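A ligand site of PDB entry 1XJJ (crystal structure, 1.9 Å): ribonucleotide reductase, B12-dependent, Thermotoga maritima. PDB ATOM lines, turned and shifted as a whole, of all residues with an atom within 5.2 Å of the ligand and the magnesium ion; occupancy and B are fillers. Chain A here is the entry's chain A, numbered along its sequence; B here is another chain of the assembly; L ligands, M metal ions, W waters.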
ATOM      1  N   ASP A 141      -0.094   7.405 -31.077  1.00  0.00           N
ATOM      2  CA  ASP A 141      -0.691   8.740 -30.950  1.00  0.00           C
ATOM      3  C   ASP A 141      -2.176   8.711 -31.387  1.00  0.00           C
ATOM      4  O   ASP A 141      -2.532   9.405 -32.330  1.00  0.00           O
ATOM      5  CB  ASP A 141       0.124   9.688 -31.838  1.00  0.00           C
ATOM      6  CG  ASP A 141      -0.113  11.154 -31.535  1.00  0.00           C
ATOM      7  OD1 ASP A 141      -0.498  11.480 -30.427  1.00  0.00           O
ATOM      8  OD2 ASP A 141       0.072  11.967 -32.462  1.00  0.00           O
ATOM      9  N   SER A 142      -3.050   7.942 -30.697  1.00  0.00           N
ATOM     10  CA  SER A 142      -4.488   8.008 -30.947  1.00  0.00           C
ATOM     11  C   SER A 142      -5.236   7.582 -29.688  1.00  0.00           C
ATOM     12  O   SER A 142      -4.711   6.814 -28.920  1.00  0.00           O
ATOM     13  CB  SER A 142      -4.922   7.154 -32.137  1.00  0.00           C
ATOM     14  OG  SER A 142      -4.698   5.796 -31.893  1.00  0.00           O
ATOM     15  N   ILE A 143      -6.458   8.084 -29.492  1.00  0.00           N
ATOM     16  CA  ILE A 143      -7.286   7.729 -28.345  1.00  0.00           C
ATOM     17  C   ILE A 143      -7.458   6.223 -28.355  1.00  0.00           C
ATOM     18  O   ILE A 143      -7.337   5.572 -27.345  1.00  0.00           O
ATOM     19  CB  ILE A 143      -8.672   8.494 -28.398  1.00  0.00           C
ATOM     20  CG1 ILE A 143      -8.438  10.018 -28.181  1.00  0.00           C
ATOM     21  CG2 ILE A 143      -9.710   7.925 -27.373  1.00  0.00           C
ATOM     22  CD1 ILE A 143      -7.845  10.455 -26.787  1.00  0.00           C
ATOM     23  N   GLU A 144      -7.672   5.650 -29.523  1.00  0.00           N
ATOM     24  CA  GLU A 144      -7.843   4.212 -29.589  1.00  0.00           C
ATOM     25  C   GLU A 144      -6.622   3.445 -29.057  1.00  0.00           C
ATOM     26  O   GLU A 144      -6.779   2.461 -28.271  1.00  0.00           O
ATOM     27  CB  GLU A 144      -8.138   3.803 -31.027  1.00  0.00           C
ATOM     28  CG  GLU A 144      -7.833   2.349 -31.472  1.00  0.00           C
ATOM     29  CD  GLU A 144      -8.840   1.304 -30.990  1.00  0.00           C
ATOM     30  OE1 GLU A 144     -10.049   1.645 -30.862  1.00  0.00           O
ATOM     31  OE2 GLU A 144      -8.416   0.129 -30.739  1.00  0.00           O
ATOM     32  N   ILE A 146      -4.112   4.657 -27.254  1.00  0.00           N
ATOM     33  CA  ILE A 146      -3.801   5.015 -25.888  1.00  0.00           C
ATOM     34  C   ILE A 146      -4.584   4.142 -24.923  1.00  0.00           C
ATOM     35  O   ILE A 146      -4.056   3.676 -23.883  1.00  0.00           O
ATOM     36  CB  ILE A 146      -4.173   6.459 -25.563  1.00  0.00           C
ATOM     37  CG1 ILE A 146      -3.053   7.394 -25.982  1.00  0.00           C
ATOM     38  CG2 ILE A 146      -4.239   6.614 -24.098  1.00  0.00           C
ATOM     39  CD1 ILE A 146      -3.565   8.741 -26.491  1.00  0.00           C
ATOM     40  N   LEU A 170       2.995  10.433 -28.256  1.00  0.00           N
ATOM     41  CA  LEU A 170       1.841  11.249 -28.001  1.00  0.00           C
ATOM     42  C   LEU A 170       2.175  12.718 -28.266  1.00  0.00           C
ATOM     43  O   LEU A 170       3.127  13.225 -27.683  1.00  0.00           O
ATOM     44  CB  LEU A 170       1.284  11.019 -26.563  1.00  0.00           C
ATOM     45  CG  LEU A 170       0.972   9.596 -26.063  1.00  0.00           C
ATOM     46  CD1 LEU A 170       0.200   9.632 -24.767  1.00  0.00           C
ATOM     47  CD2 LEU A 170       0.172   8.898 -27.132  1.00  0.00           C
ATOM     48  N   ARG A 171       1.402  13.392 -29.144  1.00  0.00           N
ATOM     49  CA  ARG A 171       1.706  14.751 -29.552  1.00  0.00           C
ATOM     50  C   ARG A 171       1.566  15.700 -28.382  1.00  0.00           C
ATOM     51  O   ARG A 171       0.727  15.469 -27.486  1.00  0.00           O
ATOM     52  CB  ARG A 171       0.829  15.188 -30.729  1.00  0.00           C
ATOM     53  CG  ARG A 171      -0.669  15.421 -30.421  1.00  0.00           C
ATOM     54  CD  ARG A 171      -1.530  15.533 -31.688  1.00  0.00           C
ATOM     55  NE  ARG A 171      -1.514  14.286 -32.507  1.00  0.00           N
ATOM     56  CZ  ARG A 171      -2.366  14.014 -33.484  1.00  0.00           C
ATOM     57  NH1 ARG A 171      -3.319  14.864 -33.798  1.00  0.00           N
ATOM     58  NH2 ARG A 171      -2.296  12.855 -34.130  1.00  0.00           N
ATOM     59  N   PHE A 176      -2.730  20.415 -32.595  1.00  0.00           N
ATOM     60  CA  PHE A 176      -3.862  20.230 -33.514  1.00  0.00           C
ATOM     61  C   PHE A 176      -4.342  18.785 -33.539  1.00  0.00           C
ATOM     62  O   PHE A 176      -3.538  17.859 -33.692  1.00  0.00           O
ATOM     63  CB  PHE A 176      -3.435  20.660 -34.919  1.00  0.00           C
ATOM     64  CG  PHE A 176      -4.521  20.530 -35.985  1.00  0.00           C
ATOM     65  CD1 PHE A 176      -5.552  21.470 -36.064  1.00  0.00           C
ATOM     66  CD2 PHE A 176      -4.487  19.492 -36.915  1.00  0.00           C
ATOM     67  CE1 PHE A 176      -6.551  21.371 -37.052  1.00  0.00           C
ATOM     68  CE2 PHE A 176      -5.453  19.369 -37.896  1.00  0.00           C
ATOM     69  CZ  PHE A 176      -6.511  20.323 -37.975  1.00  0.00           C
ATOM     70  N   VAL A 177      -5.660  18.605 -33.435  1.00  0.00           N
ATOM     71  CA  VAL A 177      -6.289  17.322 -33.715  1.00  0.00           C
ATOM     72  C   VAL A 177      -7.174  17.453 -34.953  1.00  0.00           C
ATOM     73  O   VAL A 177      -8.038  18.321 -34.970  1.00  0.00           O
ATOM     74  CB  VAL A 177      -7.157  16.826 -32.530  1.00  0.00           C
ATOM     75  CG1 VAL A 177      -7.765  15.481 -32.852  1.00  0.00           C
ATOM     76  CG2 VAL A 177      -6.321  16.770 -31.225  1.00  0.00           C
ATOM     77  N   ALA A 178      -6.997  16.602 -35.950  1.00  0.00           N
ATOM     78  CA  ALA A 178      -7.668  16.838 -37.235  1.00  0.00           C
ATOM     79  C   ALA A 178      -9.169  16.825 -37.108  1.00  0.00           C
ATOM     80  O   ALA A 178      -9.709  16.157 -36.218  1.00  0.00           O
ATOM     81  CB  ALA A 178      -7.217  15.848 -38.308  1.00  0.00           C
ATOM     82  N   LYS A 183      -7.763  20.676 -28.911  1.00  0.00           N
ATOM     83  CA  LYS A 183      -6.332  20.361 -28.928  1.00  0.00           C
ATOM     84  C   LYS A 183      -6.023  19.041 -28.173  1.00  0.00           C
ATOM     85  O   LYS A 183      -6.792  18.647 -27.294  1.00  0.00           O
ATOM     86  CB  LYS A 183      -5.580  21.508 -28.265  1.00  0.00           C
ATOM     87  CG  LYS A 183      -5.865  22.905 -28.884  1.00  0.00           C
ATOM     88  CD  LYS A 183      -5.493  22.878 -30.369  1.00  0.00           C
ATOM     89  CE  LYS A 183      -5.598  24.275 -31.034  1.00  0.00           C
ATOM     90  NZ  LYS A 183      -5.857  24.130 -32.523  1.00  0.00           N
ATOM     91  N   ALA A 184      -4.932  18.370 -28.539  1.00  0.00           N
ATOM     92  CA  ALA A 184      -4.438  17.206 -27.785  1.00  0.00           C
ATOM     93  C   ALA A 184      -3.979  17.583 -26.391  1.00  0.00           C
ATOM     94  O   ALA A 184      -3.420  18.697 -26.182  1.00  0.00           O
ATOM     95  CB  ALA A 184      -3.331  16.529 -28.543  1.00  0.00           C
ATOM     96  N   SER A 185      -4.250  16.713 -25.414  1.00  0.00           N
ATOM     97  CA  SER A 185      -3.895  17.025 -24.039  1.00  0.00           C
ATOM     98  C   SER A 185      -2.427  16.838 -23.685  1.00  0.00           C
ATOM     99  O   SER A 185      -1.932  17.486 -22.777  1.00  0.00           O
ATOM    100  CB  SER A 185      -4.787  16.262 -23.028  1.00  0.00           C
ATOM    101  OG  SER A 185      -4.890  14.891 -23.441  1.00  0.00           O
ATOM    102  N   PHE A 190      -2.310  11.836 -20.277  1.00  0.00           N
ATOM    103  CA  PHE A 190      -2.634  10.415 -20.435  1.00  0.00           C
ATOM    104  C   PHE A 190      -1.952   9.499 -19.438  1.00  0.00           C
ATOM    105  O   PHE A 190      -2.570   8.564 -18.940  1.00  0.00           O
ATOM    106  CB  PHE A 190      -2.480   9.914 -21.888  1.00  0.00           C
ATOM    107  CG  PHE A 190      -3.445  10.530 -22.817  1.00  0.00           C
ATOM    108  CD1 PHE A 190      -4.786  10.144 -22.805  1.00  0.00           C
ATOM    109  CD2 PHE A 190      -3.068  11.630 -23.631  1.00  0.00           C
ATOM    110  CE1 PHE A 190      -5.759  10.801 -23.618  1.00  0.00           C
ATOM    111  CE2 PHE A 190      -4.007  12.265 -24.458  1.00  0.00           C
ATOM    112  CZ  PHE A 190      -5.349  11.857 -24.435  1.00  0.00           C
ATOM    113  N   HIS B 127     -15.749   9.708 -39.827  1.00  0.00           N
ATOM    114  CA  HIS B 127     -15.824   8.908 -38.577  1.00  0.00           C
ATOM    115  C   HIS B 127     -16.341   9.768 -37.408  1.00  0.00           C
ATOM    116  O   HIS B 127     -16.684   9.285 -36.344  1.00  0.00           O
ATOM    117  CB  HIS B 127     -14.407   8.332 -38.286  1.00  0.00           C
ATOM    118  CG  HIS B 127     -13.395   9.397 -38.004  1.00  0.00           C
ATOM    119  ND1 HIS B 127     -12.844   9.598 -36.758  1.00  0.00           N
ATOM    120  CD2 HIS B 127     -12.904  10.391 -38.800  1.00  0.00           C
ATOM    121  CE1 HIS B 127     -12.024  10.644 -36.803  1.00  0.00           C
ATOM    122  NE2 HIS B 127     -12.059  11.151 -38.016  1.00  0.00           N
ATOM    123  N   LEU B 128     -16.347  11.086 -37.616  1.00  0.00           N
ATOM    124  CA  LEU B 128     -16.858  12.012 -36.632  1.00  0.00           C
ATOM    125  C   LEU B 128     -18.351  12.354 -36.843  1.00  0.00           C
ATOM    126  O   LEU B 128     -18.945  13.163 -36.082  1.00  0.00           O
ATOM    127  CB  LEU B 128     -16.066  13.302 -36.672  1.00  0.00           C
ATOM    128  CG  LEU B 128     -14.550  13.276 -36.425  1.00  0.00           C
ATOM    129  CD1 LEU B 128     -14.062  14.748 -36.240  1.00  0.00           C
ATOM    130  CD2 LEU B 128     -14.241  12.409 -35.156  1.00  0.00           C
ATOM    131  N   LYS B 158     -15.236  11.096 -26.935  1.00  0.00           N
ATOM    132  CA  LYS B 158     -14.497  11.828 -27.971  1.00  0.00           C
ATOM    133  C   LYS B 158     -15.398  12.303 -29.108  1.00  0.00           C
ATOM    134  O   LYS B 158     -15.319  13.452 -29.486  1.00  0.00           O
ATOM    135  CB  LYS B 158     -13.355  10.969 -28.527  1.00  0.00           C
ATOM    136  CG  LYS B 158     -12.586  11.718 -29.592  1.00  0.00           C
ATOM    137  CD  LYS B 158     -11.448  10.919 -30.209  1.00  0.00           C
ATOM    138  CE  LYS B 158     -10.831  11.790 -31.340  1.00  0.00           C
ATOM    139  NZ  LYS B 158     -10.718  10.944 -32.590  1.00  0.00           N
ATOM    140  N   VAL B 200      -9.644  13.320 -18.525  1.00  0.00           N
ATOM    141  CA  VAL B 200      -8.538  13.666 -19.411  1.00  0.00           C
ATOM    142  C   VAL B 200      -9.048  13.854 -20.846  1.00  0.00           C
ATOM    143  O   VAL B 200      -8.641  14.788 -21.534  1.00  0.00           O
ATOM    144  CB  VAL B 200      -7.412  12.587 -19.363  1.00  0.00           C
ATOM    145  CG1 VAL B 200      -6.357  12.833 -20.464  1.00  0.00           C
ATOM    146  CG2 VAL B 200      -6.750  12.622 -17.958  1.00  0.00           C
ATOM    147  N   VAL B 201      -9.936  12.969 -21.299  1.00  0.00           N
ATOM    148  CA  VAL B 201     -10.528  13.101 -22.634  1.00  0.00           C
ATOM    149  C   VAL B 201     -11.256  14.425 -22.799  1.00  0.00           C
ATOM    150  O   VAL B 201     -11.132  15.048 -23.865  1.00  0.00           O
ATOM    151  CB  VAL B 201     -11.438  11.915 -22.995  1.00  0.00           C
ATOM    152  CG1 VAL B 201     -12.125  12.189 -24.357  1.00  0.00           C
ATOM    153  CG2 VAL B 201     -10.625  10.705 -23.085  1.00  0.00           C
ATOM    154  N   LYS B 202     -11.900  14.907 -21.742  1.00  0.00           N
ATOM    155  CA  LYS B 202     -12.643  16.192 -21.768  1.00  0.00           C
ATOM    156  C   LYS B 202     -11.876  17.441 -21.291  1.00  0.00           C
ATOM    157  O   LYS B 202     -12.340  18.577 -21.422  1.00  0.00           O
ATOM    158  CB  LYS B 202     -13.948  16.032 -20.982  1.00  0.00           C
ATOM    159  CG  LYS B 202     -14.873  15.049 -21.645  1.00  0.00           C
ATOM    160  CD  LYS B 202     -16.188  14.957 -20.906  1.00  0.00           C
ATOM    161  CE  LYS B 202     -17.223  16.003 -21.365  1.00  0.00           C
ATOM    162  NZ  LYS B 202     -18.243  16.247 -20.254  1.00  0.00           N
ATOM    163  N   GLN B 203     -10.687  17.230 -20.766  1.00  0.00           N
ATOM    164  CA  GLN B 203      -9.738  18.287 -20.518  1.00  0.00           C
ATOM    165  C   GLN B 203      -9.542  19.185 -21.772  1.00  0.00           C
ATOM    166  O   GLN B 203      -8.647  18.944 -22.607  1.00  0.00           O
ATOM    167  CB  GLN B 203      -8.415  17.617 -20.176  1.00  0.00           C
ATOM    168  CG  GLN B 203      -7.326  18.542 -19.764  1.00  0.00           C
ATOM    169  CD  GLN B 203      -6.046  17.779 -19.560  1.00  0.00           C
ATOM    170  OE1 GLN B 203      -5.063  18.012 -20.273  1.00  0.00           O
ATOM    171  NE2 GLN B 203      -6.037  16.860 -18.583  1.00  0.00           N
HETATM  172  P1  LIG L   1      -5.678  13.054 -36.052  1.00  0.00           P
HETATM  173  O1  LIG L   1      -5.295  14.432 -35.844  1.00  0.00           O
HETATM  174  O2  LIG L   1      -4.893  11.953 -35.420  1.00  0.00           O
HETATM  175  O3  LIG L   1      -5.763  12.642 -37.590  1.00  0.00           O
HETATM  176  O4  LIG L   1      -7.133  12.989 -35.502  1.00  0.00           O
HETATM  177  P2  LIG L   1      -7.808  11.745 -34.820  1.00  0.00           P
HETATM  178  O5  LIG L   1      -9.253  12.131 -34.683  1.00  0.00           O
HETATM  179  O6  LIG L   1      -7.425  10.472 -35.494  1.00  0.00           O
HETATM  180  O7  LIG L   1      -7.356  11.796 -33.202  1.00  0.00           O
HETATM  181  P3  LIG L   1      -6.586  10.571 -32.408  1.00  0.00           P
HETATM  182  O8  LIG L   1      -5.666   9.852 -33.300  1.00  0.00           O
HETATM  183  O9  LIG L   1      -7.613   9.751 -31.717  1.00  0.00           O
HETATM  184  O10 LIG L   1      -5.860  11.598 -31.322  1.00  0.00           O
HETATM  185  C1  LIG L   1      -4.616  12.139 -31.616  1.00  0.00           C
HETATM  186  C2  LIG L   1      -3.825  12.645 -30.448  1.00  0.00           C
HETATM  187  O11 LIG L   1      -4.592  13.806 -29.957  1.00  0.00           O
HETATM  188  C3  LIG L   1      -3.647  11.646 -29.305  1.00  0.00           C
HETATM  189  O12 LIG L   1      -2.396  11.963 -28.620  1.00  0.00           O
HETATM  190  C4  LIG L   1      -4.902  11.896 -28.503  1.00  0.00           C
HETATM  191  C5  LIG L   1      -5.136  13.441 -28.642  1.00  0.00           C
HETATM  192  N1  LIG L   1      -6.613  13.690 -28.629  1.00  0.00           N
HETATM  193  C6  LIG L   1      -7.478  13.503 -29.655  1.00  0.00           C
HETATM  194  N2  LIG L   1      -8.714  13.774 -29.265  1.00  0.00           N
HETATM  195  C7  LIG L   1      -8.657  14.131 -27.982  1.00  0.00           C
HETATM  196  C8  LIG L   1      -9.646  14.468 -27.093  1.00  0.00           C
HETATM  197  O13 LIG L   1     -10.817  14.533 -27.472  1.00  0.00           O
HETATM  198  N3  LIG L   1      -9.285  14.797 -25.801  1.00  0.00           N
HETATM  199  C9  LIG L   1      -7.907  14.715 -25.410  1.00  0.00           C
HETATM  200  N4  LIG L   1      -7.563  15.018 -24.198  1.00  0.00           N
HETATM  201  N5  LIG L   1      -6.965  14.353 -26.303  1.00  0.00           N
HETATM  202  C10 LIG L   1      -7.330  14.057 -27.564  1.00  0.00           C
HETATM  203 MG    MG M   1      -5.377   9.959 -35.290  1.00  0.00          MG
HETATM  204  O   HOH W   1      -5.800   8.079 -35.767  1.00  0.00           O
HETATM  205  O   HOH W   2     -13.265  15.444 -26.173  1.00  0.00           O
HETATM  206  O   HOH W   3      -9.586  17.653 -27.680  1.00  0.00           O
HETATM  207  O   HOH W   4      -4.974  10.354 -37.460  1.00  0.00           O
HETATM  208  O   HOH W   5     -10.989  14.717 -31.043  1.00  0.00           O
HETATM  209  O   HOH W   6      -1.682  13.869 -27.107  1.00  0.00           O
HETATM  210  O   HOH W   7      -8.042  12.340 -38.954  1.00  0.00           O
HETATM  211  O   HOH W   8      -8.549   8.797 -37.616  1.00  0.00           O
HETATM  212  O   HOH W   9      -3.311   9.528 -34.877  1.00  0.00           O
HETATM  213  O   HOH W  10      -8.659   7.136 -31.962  1.00  0.00           O
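No residue comes within 4 Å of the magnesium ion.
The side-chain carboxylate (OD2) of Asp 141 lies within salt-bridge range of the guanidinium group (NE) of Arg 171.
The backbone carbonyl oxygen (O) of Phe 176 is in hydrogen-bond range of the guanidinium group (NH1) of Arg 171 (3.0 Å).
Ser 142 touches the ligand.
CD1 of Ile 146 touches C4 of the ligand (3.97 Å).
Val 177 touches the ligand (CG2 to O11, 3.7 Å).
Ala 184 touches the ligand.
Phe 190 touches the ligand.
His 127 of chain B touches the ligand.
Hydrophobic or aromatic side chains that line the ligand: Ile 143, Ile 146, Val 177, Ala 178, Ala 184, Phe 190 and His 127 of chain B.
14 residues have an atom within 4 Å of the ligand: Asp 141, Ser 142, Ile 143, Ile 146, Arg 171, Val 177, Ala 178, Ala 184, Ser 185, Phe 190, His 127 of chain B, Lys 158 of chain B, Val 200 of chain B and Val 201 of chain B.
Water W6 bridges an oxygen (O12) of the ligand (2.5 Å) and the backbone carbonyl oxygen (O) of Arg 171 (2.9 Å).
Water W10 lies within hydrogen-bond range of O9 of the ligand (2.8 Å), N of Glu 144 (3.0 Å) and N of Ile 143 (3.4 Å).
Water W2 lies within hydrogen-bond range of O13 of the ligand and O of Val 201 of chain B.
Water W3 bridges O of Lys 183 (3.0 Å) and O13 of the ligand (3.4 Å).
The side-chain carboxylate (OD1) of Asp 141 sits at hydrogen-bond distance from an oxygen (O12) of the ligand (2.7 Å).
A nitrogen (N3) of the ligand is in hydrogen-bond range of the backbone carbonyl oxygen of Val 201 of chain B (2.7 Å).
The backbone NH (N) of Ala 178 sits at hydrogen-bond distance from an oxygen (O1) of the ligand (2.8 Å).
N4 of the ligand is in hydrogen-bond range of OG of Ser 185.
NZ of Lys 158 of chain B is in salt-bridge range of O5 of the ligand, 2.8 Å away.
NH1 of Arg 171 lies within salt-bridge range of O1 of the ligand (2.9 Å).
A nitrogen (N4) of the ligand lies within hydrogen-bond range of the backbone carbonyl oxygen (O) of Val 200 of chain B, at 2.9 Å.
The backbone NH (N) of Ile 143 lies within hydrogen-bond range of an oxygen (O9) of the ligand, 3.0 Å away.
The magnesium ion is bound by water W1, an oxygen (O8) of the ligand, an oxygen (O2) of the ligand, an oxygen (O6) of the ligand, water W9 and water W4.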
